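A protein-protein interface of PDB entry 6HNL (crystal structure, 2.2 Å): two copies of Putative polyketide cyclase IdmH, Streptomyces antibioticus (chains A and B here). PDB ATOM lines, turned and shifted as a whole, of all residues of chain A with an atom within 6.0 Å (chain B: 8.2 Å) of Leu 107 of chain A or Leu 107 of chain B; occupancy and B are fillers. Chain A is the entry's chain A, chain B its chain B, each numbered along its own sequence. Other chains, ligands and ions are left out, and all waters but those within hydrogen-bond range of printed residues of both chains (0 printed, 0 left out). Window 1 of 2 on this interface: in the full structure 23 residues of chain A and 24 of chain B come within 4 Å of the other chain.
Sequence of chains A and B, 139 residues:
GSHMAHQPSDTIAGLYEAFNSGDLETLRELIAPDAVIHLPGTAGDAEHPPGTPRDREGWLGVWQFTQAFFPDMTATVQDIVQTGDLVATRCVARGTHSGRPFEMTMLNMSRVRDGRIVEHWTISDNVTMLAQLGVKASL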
ATOM      1  N   THR A  89      16.328 -18.789   4.737  1.00  0.00           N
ATOM      2  CA  THR A  89      15.393 -19.883   4.497  1.00  0.00           C
ATOM      3  C   THR A  89      15.962 -21.223   4.920  1.00  0.00           C
ATOM      4  O   THR A  89      17.174 -21.482   4.763  1.00  0.00           O
ATOM      5  CB  THR A  89      15.006 -20.012   3.012  1.00  0.00           C
ATOM      6  OG1 THR A  89      16.180 -19.982   2.196  1.00  0.00           O
ATOM      7  CG2 THR A  89      14.093 -18.877   2.598  1.00  0.00           C
ATOM      8  N   ARG A  90      15.083 -22.071   5.447  1.00  0.00           N
ATOM      9  CA  ARG A  90      15.370 -23.478   5.627  1.00  0.00           C
ATOM     10  C   ARG A  90      14.572 -24.209   4.573  1.00  0.00           C
ATOM     11  O   ARG A  90      13.351 -24.028   4.485  1.00  0.00           O
ATOM     12  CB  ARG A  90      14.973 -23.965   7.017  1.00  0.00           C
ATOM     13  CG  ARG A  90      15.218 -25.446   7.214  1.00  0.00           C
ATOM     14  CD  ARG A  90      14.960 -25.895   8.629  1.00  0.00           C
ATOM     15  NE  ARG A  90      13.562 -25.768   9.012  1.00  0.00           N
ATOM     16  CZ  ARG A  90      12.589 -26.645   8.739  1.00  0.00           C
ATOM     17  NH1 ARG A  90      12.817 -27.753   8.028  1.00  0.00           N
ATOM     18  NH2 ARG A  90      11.358 -26.396   9.195  1.00  0.00           N
ATOM     19  N   CYS A  91      15.264 -25.017   3.767  1.00  0.00           N
ATOM     20  CA  CYS A  91      14.638 -25.815   2.740  1.00  0.00           C
ATOM     21  C   CYS A  91      14.903 -27.279   2.985  1.00  0.00           C
ATOM     22  O   CYS A  91      15.890 -27.643   3.639  1.00  0.00           O
ATOM     23  CB  CYS A  91      15.183 -25.469   1.360  1.00  0.00           C
ATOM     24  SG  CYS A  91      14.998 -23.761   0.867  1.00  0.00           S
ATOM     25  N   THR A 105      18.407 -31.339   4.525  1.00  0.00           N
ATOM     26  CA  THR A 105      18.218 -29.962   4.928  1.00  0.00           C
ATOM     27  C   THR A 105      19.185 -29.055   4.164  1.00  0.00           C
ATOM     28  O   THR A 105      20.323 -29.445   3.860  1.00  0.00           O
ATOM     29  CB  THR A 105      18.388 -29.821   6.449  1.00  0.00           C
ATOM     30  OG1 THR A 105      17.391 -30.616   7.095  1.00  0.00           O
ATOM     31  CG2 THR A 105      18.236 -28.363   6.911  1.00  0.00           C
ATOM     32  N   MET A 106      18.695 -27.873   3.797  1.00  0.00           N
ATOM     33  CA  MET A 106      19.522 -26.795   3.247  1.00  0.00           C
ATOM     34  C   MET A 106      19.215 -25.531   4.003  1.00  0.00           C
ATOM     35  O   MET A 106      18.056 -25.257   4.325  1.00  0.00           O
ATOM     36  CB  MET A 106      19.253 -26.457   1.789  1.00  0.00           C
ATOM     37  CG  MET A 106      18.997 -27.646   0.869  1.00  0.00           C
ATOM     38  SD  MET A 106      18.571 -27.013  -0.949  1.00  0.00           S
ATOM     39  CE  MET A 106      19.424 -25.222  -1.010  1.00  0.00           C
ATOM     40  N   LEU A 107      20.247 -24.740   4.282  1.00  0.00           N
ATOM     41  CA  LEU A 107      20.087 -23.445   4.918  1.00  0.00           C
ATOM     42  C   LEU A 107      20.679 -22.410   3.981  1.00  0.00           C
ATOM     43  O   LEU A 107      21.761 -22.610   3.425  1.00  0.00           O
ATOM     44  CB  LEU A 107      20.785 -23.410   6.270  1.00  0.00           C
ATOM     45  CG  LEU A 107      20.205 -24.332   7.339  1.00  0.00           C
ATOM     46  CD1 LEU A 107      21.046 -24.218   8.592  1.00  0.00           C
ATOM     47  CD2 LEU A 107      18.757 -23.998   7.662  1.00  0.00           C
ATOM     48  N   ASN A 108      19.961 -21.310   3.804  1.00  0.00           N
ATOM     49  CA  ASN A 108      20.337 -20.269   2.871  1.00  0.00           C
ATOM     50  C   ASN A 108      20.144 -18.921   3.521  1.00  0.00           C
ATOM     51  O   ASN A 108      19.315 -18.778   4.415  1.00  0.00           O
ATOM     52  CB  ASN A 108      19.476 -20.325   1.619  1.00  0.00           C
ATOM     53  CG  ASN A 108      19.279 -21.734   1.115  1.00  0.00           C
ATOM     54  OD1 ASN A 108      20.191 -22.338   0.545  1.00  0.00           O
ATOM     55  ND2 ASN A 108      18.079 -22.267   1.324  1.00  0.00           N
ATOM     56  N   MET A 109      20.902 -17.949   3.045  1.00  0.00           N
ATOM     57  CA  MET A 109      20.713 -16.559   3.441  1.00  0.00           C
ATOM     58  C   MET A 109      20.988 -15.730   2.237  1.00  0.00           C
ATOM     59  O   MET A 109      21.999 -15.910   1.584  1.00  0.00           O
ATOM     60  CB  MET A 109      21.594 -16.131   4.600  1.00  0.00           C
ATOM     61  CG  MET A 109      21.002 -14.820   5.114  1.00  0.00           C
ATOM     62  SD  MET A 109      22.145 -14.237   6.557  1.00  0.00           S
ATOM     63  CE  MET A 109      21.143 -15.244   7.933  1.00  0.00           C
ATOM     64  N   TRP A 121      24.368 -16.928   0.590  1.00  0.00           N
ATOM     65  CA  TRP A 121      25.129 -17.975   1.246  1.00  0.00           C
ATOM     66  C   TRP A 121      24.235 -19.207   1.287  1.00  0.00           C
ATOM     67  O   TRP A 121      23.037 -19.079   1.584  1.00  0.00           O
ATOM     68  CB  TRP A 121      25.475 -17.589   2.678  1.00  0.00           C
ATOM     69  CG  TRP A 121      26.372 -16.395   2.844  1.00  0.00           C
ATOM     70  CD1 TRP A 121      27.732 -16.409   3.039  1.00  0.00           C
ATOM     71  CD2 TRP A 121      25.979 -15.019   2.865  1.00  0.00           C
ATOM     72  NE1 TRP A 121      28.199 -15.124   3.170  1.00  0.00           N
ATOM     73  CE2 TRP A 121      27.145 -14.255   3.066  1.00  0.00           C
ATOM     74  CE3 TRP A 121      24.752 -14.359   2.726  1.00  0.00           C
ATOM     75  CZ2 TRP A 121      27.128 -12.859   3.126  1.00  0.00           C
ATOM     76  CZ3 TRP A 121      24.727 -12.963   2.789  1.00  0.00           C
ATOM     77  CH2 TRP A 121      25.914 -12.227   2.986  1.00  0.00           C
ATOM     78  N   THR A 122      24.793 -20.380   0.990  1.00  0.00           N
ATOM     79  CA  THR A 122      24.046 -21.644   1.099  1.00  0.00           C
ATOM     80  C   THR A 122      24.960 -22.779   1.577  1.00  0.00           C
ATOM     81  O   THR A 122      26.148 -22.800   1.253  1.00  0.00           O
ATOM     82  CB  THR A 122      23.327 -22.021  -0.213  1.00  0.00           C
ATOM     83  OG1 THR A 122      22.537 -23.211  -0.024  1.00  0.00           O
ATOM     84  CG2 THR A 122      24.299 -22.253  -1.355  1.00  0.00           C
ATOM     85  N   ILE A 123      24.411 -23.678   2.386  1.00  0.00           N
ATOM     86  CA  ILE A 123      25.092 -24.916   2.756  1.00  0.00           C
ATOM     87  C   ILE A 123      24.033 -26.015   2.828  1.00  0.00           C
ATOM     88  O   ILE A 123      22.930 -25.793   3.347  1.00  0.00           O
ATOM     89  CB  ILE A 123      25.832 -24.843   4.119  1.00  0.00           C
ATOM     90  CG1 ILE A 123      26.700 -23.581   4.231  1.00  0.00           C
ATOM     91  CG2 ILE A 123      26.723 -26.068   4.294  1.00  0.00           C
ATOM     92  CD1 ILE A 123      27.461 -23.443   5.535  1.00  0.00           C
ATOM     93  N   SER A 124      24.375 -27.189   2.307  1.00  0.00           N
ATOM     94  CA  SER A 124      23.488 -28.346   2.321  1.00  0.00           C
ATOM     95  C   SER A 124      24.087 -29.468   3.147  1.00  0.00           C
ATOM     96  O   SER A 124      25.312 -29.601   3.251  1.00  0.00           O
ATOM     97  CB  SER A 124      23.267 -28.836   0.899  1.00  0.00           C
ATOM     98  OG  SER A 124      22.521 -27.891   0.166  1.00  0.00           O
ATOM     99  N   TYR B  16      25.657 -18.141  21.443  1.00  0.00           N
ATOM    100  CA  TYR B  16      26.988 -18.214  20.848  1.00  0.00           C
ATOM    101  C   TYR B  16      28.064 -17.627  21.773  1.00  0.00           C
ATOM    102  O   TYR B  16      29.160 -18.191  21.857  1.00  0.00           O
ATOM    103  CB  TYR B  16      26.999 -17.631  19.425  1.00  0.00           C
ATOM    104  CG  TYR B  16      26.228 -18.556  18.490  1.00  0.00           C
ATOM    105  CD1 TYR B  16      26.722 -19.822  18.177  1.00  0.00           C
ATOM    106  CD2 TYR B  16      24.981 -18.196  17.981  1.00  0.00           C
ATOM    107  CE1 TYR B  16      26.015 -20.692  17.365  1.00  0.00           C
ATOM    108  CE2 TYR B  16      24.267 -19.060  17.158  1.00  0.00           C
ATOM    109  CZ  TYR B  16      24.780 -20.302  16.859  1.00  0.00           C
ATOM    110  OH  TYR B  16      24.081 -21.162  16.054  1.00  0.00           O
ATOM    111  N   HIS B  38      18.652 -30.403  15.275  1.00  0.00           N
ATOM    112  CA  HIS B  38      18.988 -31.047  14.019  1.00  0.00           C
ATOM    113  C   HIS B  38      20.433 -30.707  13.654  1.00  0.00           C
ATOM    114  O   HIS B  38      20.735 -29.596  13.207  1.00  0.00           O
ATOM    115  CB  HIS B  38      18.033 -30.581  12.930  1.00  0.00           C
ATOM    116  CG  HIS B  38      16.584 -30.796  13.259  1.00  0.00           C
ATOM    117  ND1 HIS B  38      15.939 -32.000  13.055  1.00  0.00           N
ATOM    118  CD2 HIS B  38      15.653 -29.954  13.778  1.00  0.00           C
ATOM    119  CE1 HIS B  38      14.671 -31.878  13.412  1.00  0.00           C
ATOM    120  NE2 HIS B  38      14.472 -30.649  13.857  1.00  0.00           N
ATOM    121  N   PRO B  40      24.060 -31.632  11.492  1.00  0.00           N
ATOM    122  CA  PRO B  40      24.350 -32.172  10.165  1.00  0.00           C
ATOM    123  C   PRO B  40      24.927 -33.587  10.234  1.00  0.00           C
ATOM    124  O   PRO B  40      25.388 -34.030  11.296  1.00  0.00           O
ATOM    125  CB  PRO B  40      25.384 -31.195   9.595  1.00  0.00           C
ATOM    126  CG  PRO B  40      26.036 -30.566  10.782  1.00  0.00           C
ATOM    127  CD  PRO B  40      25.076 -30.651  11.931  1.00  0.00           C
ATOM    128  N   ASP B  79      25.439 -12.057  10.684  1.00  0.00           N
ATOM    129  CA  ASP B  79      24.110 -11.612  10.300  1.00  0.00           C
ATOM    130  C   ASP B  79      23.066 -12.333  11.139  1.00  0.00           C
ATOM    131  O   ASP B  79      23.229 -13.500  11.466  1.00  0.00           O
ATOM    132  CB  ASP B  79      23.834 -11.923   8.809  1.00  0.00           C
ATOM    133  CG  ASP B  79      24.323 -10.824   7.865  1.00  0.00           C
ATOM    134  OD1 ASP B  79      24.200  -9.614   8.197  1.00  0.00           O
ATOM    135  OD2 ASP B  79      24.821 -11.185   6.780  1.00  0.00           O
ATOM    136  N   VAL B  87      14.620 -17.298  14.443  1.00  0.00           N
ATOM    137  CA  VAL B  87      15.841 -16.509  14.253  1.00  0.00           C
ATOM    138  C   VAL B  87      16.781 -17.316  13.367  1.00  0.00           C
ATOM    139  O   VAL B  87      17.068 -18.471  13.669  1.00  0.00           O
ATOM    140  CB  VAL B  87      16.547 -16.235  15.592  1.00  0.00           C
ATOM    141  CG1 VAL B  87      17.749 -15.322  15.396  1.00  0.00           C
ATOM    142  CG2 VAL B  87      15.593 -15.598  16.585  1.00  0.00           C
ATOM    143  N   ALA B  88      17.232 -16.727  12.268  1.00  0.00           N
ATOM    144  CA  ALA B  88      18.298 -17.318  11.482  1.00  0.00           C
ATOM    145  C   ALA B  88      19.556 -16.490  11.674  1.00  0.00           C
ATOM    146  O   ALA B  88      19.484 -15.271  11.856  1.00  0.00           O
ATOM    147  CB  ALA B  88      17.919 -17.401  10.022  1.00  0.00           C
ATOM    148  N   THR B  89      20.704 -17.166  11.668  1.00  0.00           N
ATOM    149  CA  THR B  89      22.003 -16.513  11.854  1.00  0.00           C
ATOM    150  C   THR B  89      23.049 -17.078  10.916  1.00  0.00           C
ATOM    151  O   THR B  89      23.057 -18.272  10.620  1.00  0.00           O
ATOM    152  CB  THR B  89      22.545 -16.662  13.289  1.00  0.00           C
ATOM    153  OG1 THR B  89      22.443 -18.019  13.711  1.00  0.00           O
ATOM    154  CG2 THR B  89      21.774 -15.823  14.246  1.00  0.00           C
ATOM    155  N   ARG B  90      23.919 -16.194  10.448  1.00  0.00           N
ATOM    156  CA  ARG B  90      25.144 -16.575   9.788  1.00  0.00           C
ATOM    157  C   ARG B  90      26.261 -16.267  10.758  1.00  0.00           C
ATOM    158  O   ARG B  90      26.363 -15.139  11.225  1.00  0.00           O
ATOM    159  CB  ARG B  90      25.345 -15.795   8.491  1.00  0.00           C
ATOM    160  CG  ARG B  90      26.656 -16.133   7.784  1.00  0.00           C
ATOM    161  CD  ARG B  90      26.661 -15.561   6.376  1.00  0.00           C
ATOM    162  NE  ARG B  90      26.684 -14.101   6.405  1.00  0.00           N
ATOM    163  CZ  ARG B  90      27.782 -13.347   6.523  1.00  0.00           C
ATOM    164  NH1 ARG B  90      29.001 -13.887   6.634  1.00  0.00           N
ATOM    165  NH2 ARG B  90      27.658 -12.029   6.555  1.00  0.00           N
ATOM    166  N   CYS B  91      27.072 -17.269  11.077  1.00  0.00           N
ATOM    167  CA  CYS B  91      28.240 -17.088  11.931  1.00  0.00           C
ATOM    168  C   CYS B  91      29.495 -17.480  11.182  1.00  0.00           C
ATOM    169  O   CYS B  91      29.450 -18.232  10.212  1.00  0.00           O
ATOM    170  CB  CYS B  91      28.148 -17.962  13.184  1.00  0.00           C
ATOM    171  SG  CYS B  91      26.708 -17.648  14.219  1.00  0.00           S
ATOM    172  N   VAL B  92      30.619 -16.976  11.661  1.00  0.00           N
ATOM    173  CA  VAL B  92      31.936 -17.426  11.208  1.00  0.00           C
ATOM    174  C   VAL B  92      32.627 -18.090  12.396  1.00  0.00           C
ATOM    175  O   VAL B  92      32.745 -17.503  13.470  1.00  0.00           O
ATOM    176  CB  VAL B  92      32.773 -16.296  10.586  1.00  0.00           C
ATOM    177  CG1 VAL B  92      33.230 -15.271  11.625  1.00  0.00           C
ATOM    178  CG2 VAL B  92      33.973 -16.863   9.833  1.00  0.00           C
ATOM    179  N   MET B 104      35.401 -20.559   8.869  1.00  0.00           N
ATOM    180  CA  MET B 104      34.347 -21.406   8.310  1.00  0.00           C
ATOM    181  C   MET B 104      32.990 -20.794   8.557  1.00  0.00           C
ATOM    182  O   MET B 104      32.681 -20.368   9.674  1.00  0.00           O
ATOM    183  CB  MET B 104      34.489 -22.744   9.004  1.00  0.00           C
ATOM    184  CG  MET B 104      33.189 -23.527   8.996  1.00  0.00           C
ATOM    185  SD  MET B 104      33.611 -25.358   9.518  1.00  0.00           S
ATOM    186  CE  MET B 104      33.219 -25.441  11.438  1.00  0.00           C
ATOM    187  N   THR B 105      32.162 -20.783   7.519  1.00  0.00           N
ATOM    188  CA  THR B 105      30.809 -20.261   7.632  1.00  0.00           C
ATOM    189  C   THR B 105      29.922 -21.300   8.326  1.00  0.00           C
ATOM    190  O   THR B 105      30.097 -22.501   8.139  1.00  0.00           O
ATOM    191  CB  THR B 105      30.265 -19.860   6.249  1.00  0.00           C
ATOM    192  OG1 THR B 105      31.079 -18.806   5.739  1.00  0.00           O
ATOM    193  CG2 THR B 105      28.815 -19.364   6.333  1.00  0.00           C
ATOM    194  N   MET B 106      29.019 -20.810   9.165  1.00  0.00           N
ATOM    195  CA  MET B 106      27.961 -21.620   9.767  1.00  0.00           C
ATOM    196  C   MET B 106      26.645 -20.925   9.537  1.00  0.00           C
ATOM    197  O   MET B 106      26.556 -19.717   9.674  1.00  0.00           O
ATOM    198  CB  MET B 106      28.060 -21.833  11.276  1.00  0.00           C
ATOM    199  CG  MET B 106      29.461 -22.044  11.821  1.00  0.00           C
ATOM    200  SD  MET B 106      29.381 -21.997  13.818  1.00  0.00           S
ATOM    201  CE  MET B 106      27.565 -22.664  14.189  1.00  0.00           C
ATOM    202  N   LEU B 107      25.622 -21.700   9.207  1.00  0.00           N
ATOM    203  CA  LEU B 107      24.266 -21.187   9.058  1.00  0.00           C
ATOM    204  C   LEU B 107      23.385 -21.929  10.029  1.00  0.00           C
ATOM    205  O   LEU B 107      23.496 -23.143  10.167  1.00  0.00           O
ATOM    206  CB  LEU B 107      23.768 -21.383   7.628  1.00  0.00           C
ATOM    207  CG  LEU B 107      24.508 -20.594   6.559  1.00  0.00           C
ATOM    208  CD1 LEU B 107      23.925 -20.986   5.218  1.00  0.00           C
ATOM    209  CD2 LEU B 107      24.413 -19.095   6.781  1.00  0.00           C
ATOM    210  N   ASN B 108      22.534 -21.180  10.725  1.00  0.00           N
ATOM    211  CA  ASN B 108      21.720 -21.715  11.802  1.00  0.00           C
ATOM    212  C   ASN B 108      20.316 -21.165  11.672  1.00  0.00           C
ATOM    213  O   ASN B 108      20.121 -20.069  11.153  1.00  0.00           O
ATOM    214  CB  ASN B 108      22.281 -21.316  13.160  1.00  0.00           C
ATOM    215  CG  ASN B 108      23.790 -21.442  13.225  1.00  0.00           C
ATOM    216  OD1 ASN B 108      24.326 -22.546  13.292  1.00  0.00           O
ATOM    217  ND2 ASN B 108      24.481 -20.318  13.206  1.00  0.00           N
ATOM    218  N   MET B 109      19.348 -21.942  12.149  1.00  0.00           N
ATOM    219  CA  MET B 109      17.964 -21.499  12.273  1.00  0.00           C
ATOM    220  C   MET B 109      17.462 -22.026  13.579  1.00  0.00           C
ATOM    221  O   MET B 109      17.622 -23.205  13.882  1.00  0.00           O
ATOM    222  CB  MET B 109      17.195 -22.050  11.094  1.00  0.00           C
ATOM    223  CG  MET B 109      15.673 -21.921  11.141  1.00  0.00           C
ATOM    224  SD  MET B 109      15.085 -20.189  10.408  1.00  0.00           S
ATOM    225  CE  MET B 109      15.645 -20.299   8.517  1.00  0.00           C
ATOM    226  N   SER B 110      16.852 -21.154  14.359  1.00  0.00           N
ATOM    227  CA  SER B 110      16.447 -21.498  15.712  1.00  0.00           C
ATOM    228  C   SER B 110      15.019 -21.026  15.987  1.00  0.00           C
ATOM    229  O   SER B 110      14.627 -19.954  15.543  1.00  0.00           O
ATOM    230  CB  SER B 110      17.403 -20.853  16.725  1.00  0.00           C
ATOM    231  OG  SER B 110      18.764 -21.086  16.395  1.00  0.00           O
ATOM    232  N   HIS B 120      16.374 -26.181  16.736  1.00  0.00           N
ATOM    233  CA  HIS B 120      17.588 -25.628  16.138  1.00  0.00           C
ATOM    234  C   HIS B 120      18.054 -26.501  14.972  1.00  0.00           C
ATOM    235  O   HIS B 120      18.055 -27.725  15.072  1.00  0.00           O
ATOM    236  CB  HIS B 120      18.670 -25.562  17.213  1.00  0.00           C
ATOM    237  CG  HIS B 120      19.909 -24.835  16.800  1.00  0.00           C
ATOM    238  ND1 HIS B 120      19.983 -23.461  16.738  1.00  0.00           N
ATOM    239  CD2 HIS B 120      21.149 -25.293  16.506  1.00  0.00           C
ATOM    240  CE1 HIS B 120      21.207 -23.106  16.390  1.00  0.00           C
ATOM    241  NE2 HIS B 120      21.931 -24.200  16.237  1.00  0.00           N
ATOM    242  N   TRP B 121      18.393 -25.859  13.858  1.00  0.00           N
ATOM    243  CA  TRP B 121      19.055 -26.492  12.734  1.00  0.00           C
ATOM    244  C   TRP B 121      20.377 -25.757  12.549  1.00  0.00           C
ATOM    245  O   TRP B 121      20.412 -24.524  12.634  1.00  0.00           O
ATOM    246  CB  TRP B 121      18.234 -26.327  11.458  1.00  0.00           C
ATOM    247  CG  TRP B 121      16.887 -27.003  11.445  1.00  0.00           C
ATOM    248  CD1 TRP B 121      16.586 -28.218  10.896  1.00  0.00           C
ATOM    249  CD2 TRP B 121      15.661 -26.486  11.970  1.00  0.00           C
ATOM    250  NE1 TRP B 121      15.252 -28.491  11.054  1.00  0.00           N
ATOM    251  CE2 TRP B 121      14.658 -27.440  11.703  1.00  0.00           C
ATOM    252  CE3 TRP B 121      15.312 -25.306  12.635  1.00  0.00           C
ATOM    253  CZ2 TRP B 121      13.329 -27.258  12.091  1.00  0.00           C
ATOM    254  CZ3 TRP B 121      13.985 -25.112  13.012  1.00  0.00           C
ATOM    255  CH2 TRP B 121      13.010 -26.085  12.738  1.00  0.00           C
ATOM    256  N   THR B 122      21.451 -26.501  12.291  1.00  0.00           N
ATOM    257  CA  THR B 122      22.757 -25.913  11.983  1.00  0.00           C
ATOM    258  C   THR B 122      23.509 -26.747  10.949  1.00  0.00           C
ATOM    259  O   THR B 122      23.368 -27.956  10.903  1.00  0.00           O
ATOM    260  CB  THR B 122      23.614 -25.695  13.256  1.00  0.00           C
ATOM    261  OG1 THR B 122      24.835 -25.022  12.923  1.00  0.00           O
ATOM    262  CG2 THR B 122      23.948 -27.005  13.957  1.00  0.00           C
ATOM    263  N   ILE B 123      24.260 -26.074  10.081  1.00  0.00           N
ATOM    264  CA  ILE B 123      25.177 -26.736   9.155  1.00  0.00           C
ATOM    265  C   ILE B 123      26.426 -25.867   9.041  1.00  0.00           C
ATOM    266  O   ILE B 123      26.321 -24.644   8.987  1.00  0.00           O
ATOM    267  CB  ILE B 123      24.580 -26.957   7.740  1.00  0.00           C
ATOM    268  CG1 ILE B 123      23.160 -27.546   7.796  1.00  0.00           C
ATOM    269  CG2 ILE B 123      25.473 -27.898   6.946  1.00  0.00           C
ATOM    270  CD1 ILE B 123      22.522 -27.756   6.434  1.00  0.00           C
ATOM    271  N   SER B 124      27.588 -26.512   9.007  1.00  0.00           N
ATOM    272  CA  SER B 124      28.865 -25.847   8.854  1.00  0.00           C
ATOM    273  C   SER B 124      29.538 -26.227   7.550  1.00  0.00           C
ATOM    274  O   SER B 124      29.377 -27.343   7.056  1.00  0.00           O
ATOM    275  CB  SER B 124      29.777 -26.211  10.020  1.00  0.00           C
ATOM    276  OG  SER B 124      29.302 -25.581  11.187  1.00  0.00           O
ATOM    277  N   ASP B 125      30.340 -25.298   7.036  1.00  0.00           N
ATOM    278  CA  ASP B 125      31.076 -25.490   5.797  1.00  0.00           C
ATOM    279  C   ASP B 125      32.422 -26.213   6.069  1.00  0.00           C
ATOM    280  O   ASP B 125      33.498 -25.624   5.939  1.00  0.00           O
ATOM    281  CB  ASP B 125      31.284 -24.124   5.138  1.00  0.00           C
ATOM    282  CG  ASP B 125      31.746 -24.225   3.688  1.00  0.00           C
ATOM    283  OD1 ASP B 125      31.809 -25.335   3.122  1.00  0.00           O
ATOM    284  OD2 ASP B 125      32.051 -23.169   3.099  1.00  0.00           O
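O of Thr 89 of chain A lies within hydrogen-bond range of N of Asn 108 of chain A, 3.0 Å away.
The backbone carbonyl oxygen (O) of Met 109 of chain A sits at hydrogen-bond distance from the backbone NH (N) of Trp 121 of chain A (2.8 Å).
O of Thr 89 of chain B is in hydrogen-bond range of N of Asn 108 of chain B (3.0 Å).
The side-chain amide nitrogen of Asn 108 of chain B is in hydrogen-bond range of the side-chain sulfur of Cys 91 of chain B.
N of Ile 123 of chain B is in hydrogen-bond range of O of Leu 107 of chain B (3.0 Å).
The backbone carbonyl oxygen of Met 109 of chain B lies within hydrogen-bond range of the backbone NH of Trp 121 of chain B (2.8 Å).
Printed residues of chain B within 4 Å of Leu 107 of chain A: Leu 107 (3.1 Å), Asn 108 (3.999 Å) and Ile 123 (3.999 Å).
Of chain A, only Leu 107 and Ile 123 come within 4 Å of Leu 107 of chain B.
No residue of chain B comes within 4 Å of Asn 108 of chain A.
Printed residues of chain B within 4 Å of Met 109 of chain A: Asp 79, Thr 89 and Arg 90.
Printed residues of chain B within 4 Å of Trp 121 of chain A: Arg 90 (3.4 Å).
Of the printed residues of chain A, Asp 79 of chain B touches Met 109.
Of the printed residues of chain A, Asn 108 of chain B touches Leu 107.
The nearest printed residue of chain A that does not touch Leu 107 of chain B is Thr 122 of chain A (4.2 Å).
The nearest printed residue of chain B that does not touch Thr 105 of chain A is Trp 121 of chain B (4.3 Å).
Among the printed residues, pairs that only touch across the chains: Thr 89 of chain A with Met 109 of chain B (3.7 Å), Arg 90 of chain A with Met 109 of chain B (3.6 Å), Arg 90 of chain A with Trp 121 of chain B (3.4 Å), Thr 105 of chain A with Ile 123 of chain B (3.8 Å), Leu 107 of chain A with Leu 107 of chain B (3.1 Å), Leu 107 of chain A with Asn 108 of chain B (3.999 Å), Leu 107 of chain A with Ile 123 of chain B (3.999 Å), Met 109 of chain A with Asp 79 of chain B (3.6 Å), Met 109 of chain A with Thr 89 of chain B (3.99 Å), Met 109 of chain A with Arg 90 of chain B (3.9 Å), Trp 121 of chain A with Arg 90 of chain B (3.4 Å), Ile 123 of chain A with Thr 105 of chain B (3.8 Å), Ile 123 of chain A with Leu 107 of chain B (3.9 Å), Ile 123 of chain A with Ile 123 of chain B (3.5 Å) and Ile 123 of chain A with Asp 125 of chain B (3.7 Å).
Arg 90 of chain A touches Met 109 of chain B, and with the chains exchanged Met 109 of chain A touches Arg 90 of chain B.
Arg 90 of chain A touches Trp 121 of chain B, and with the chains exchanged Trp 121 of chain A touches Arg 90 of chain B.
Leu 107 of chain A touches Ile 123 of chain B, and with the chains exchanged Ile 123 of chain A touches Leu 107 of chain B.
Ile 123 of chain A touches its own counterpart, Ile 123 of chain B.
Of the 15 pairs that touch across the chains among the printed residues, 12 have their exchanged pair printed and touching as well.
Of the 12 printed residues of chain A, 7 touch a printed residue of chain B.
Hydrophobic or aromatic side chains of chain B within 4 Å of the printed part of chain A: Leu 107, Met 109, Trp 121 and Ile 123.
Among the printed residues, no Asp or Glu carboxylate lies within 4 Å of a Lys or Arg side-chain nitrogen of the other chain.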
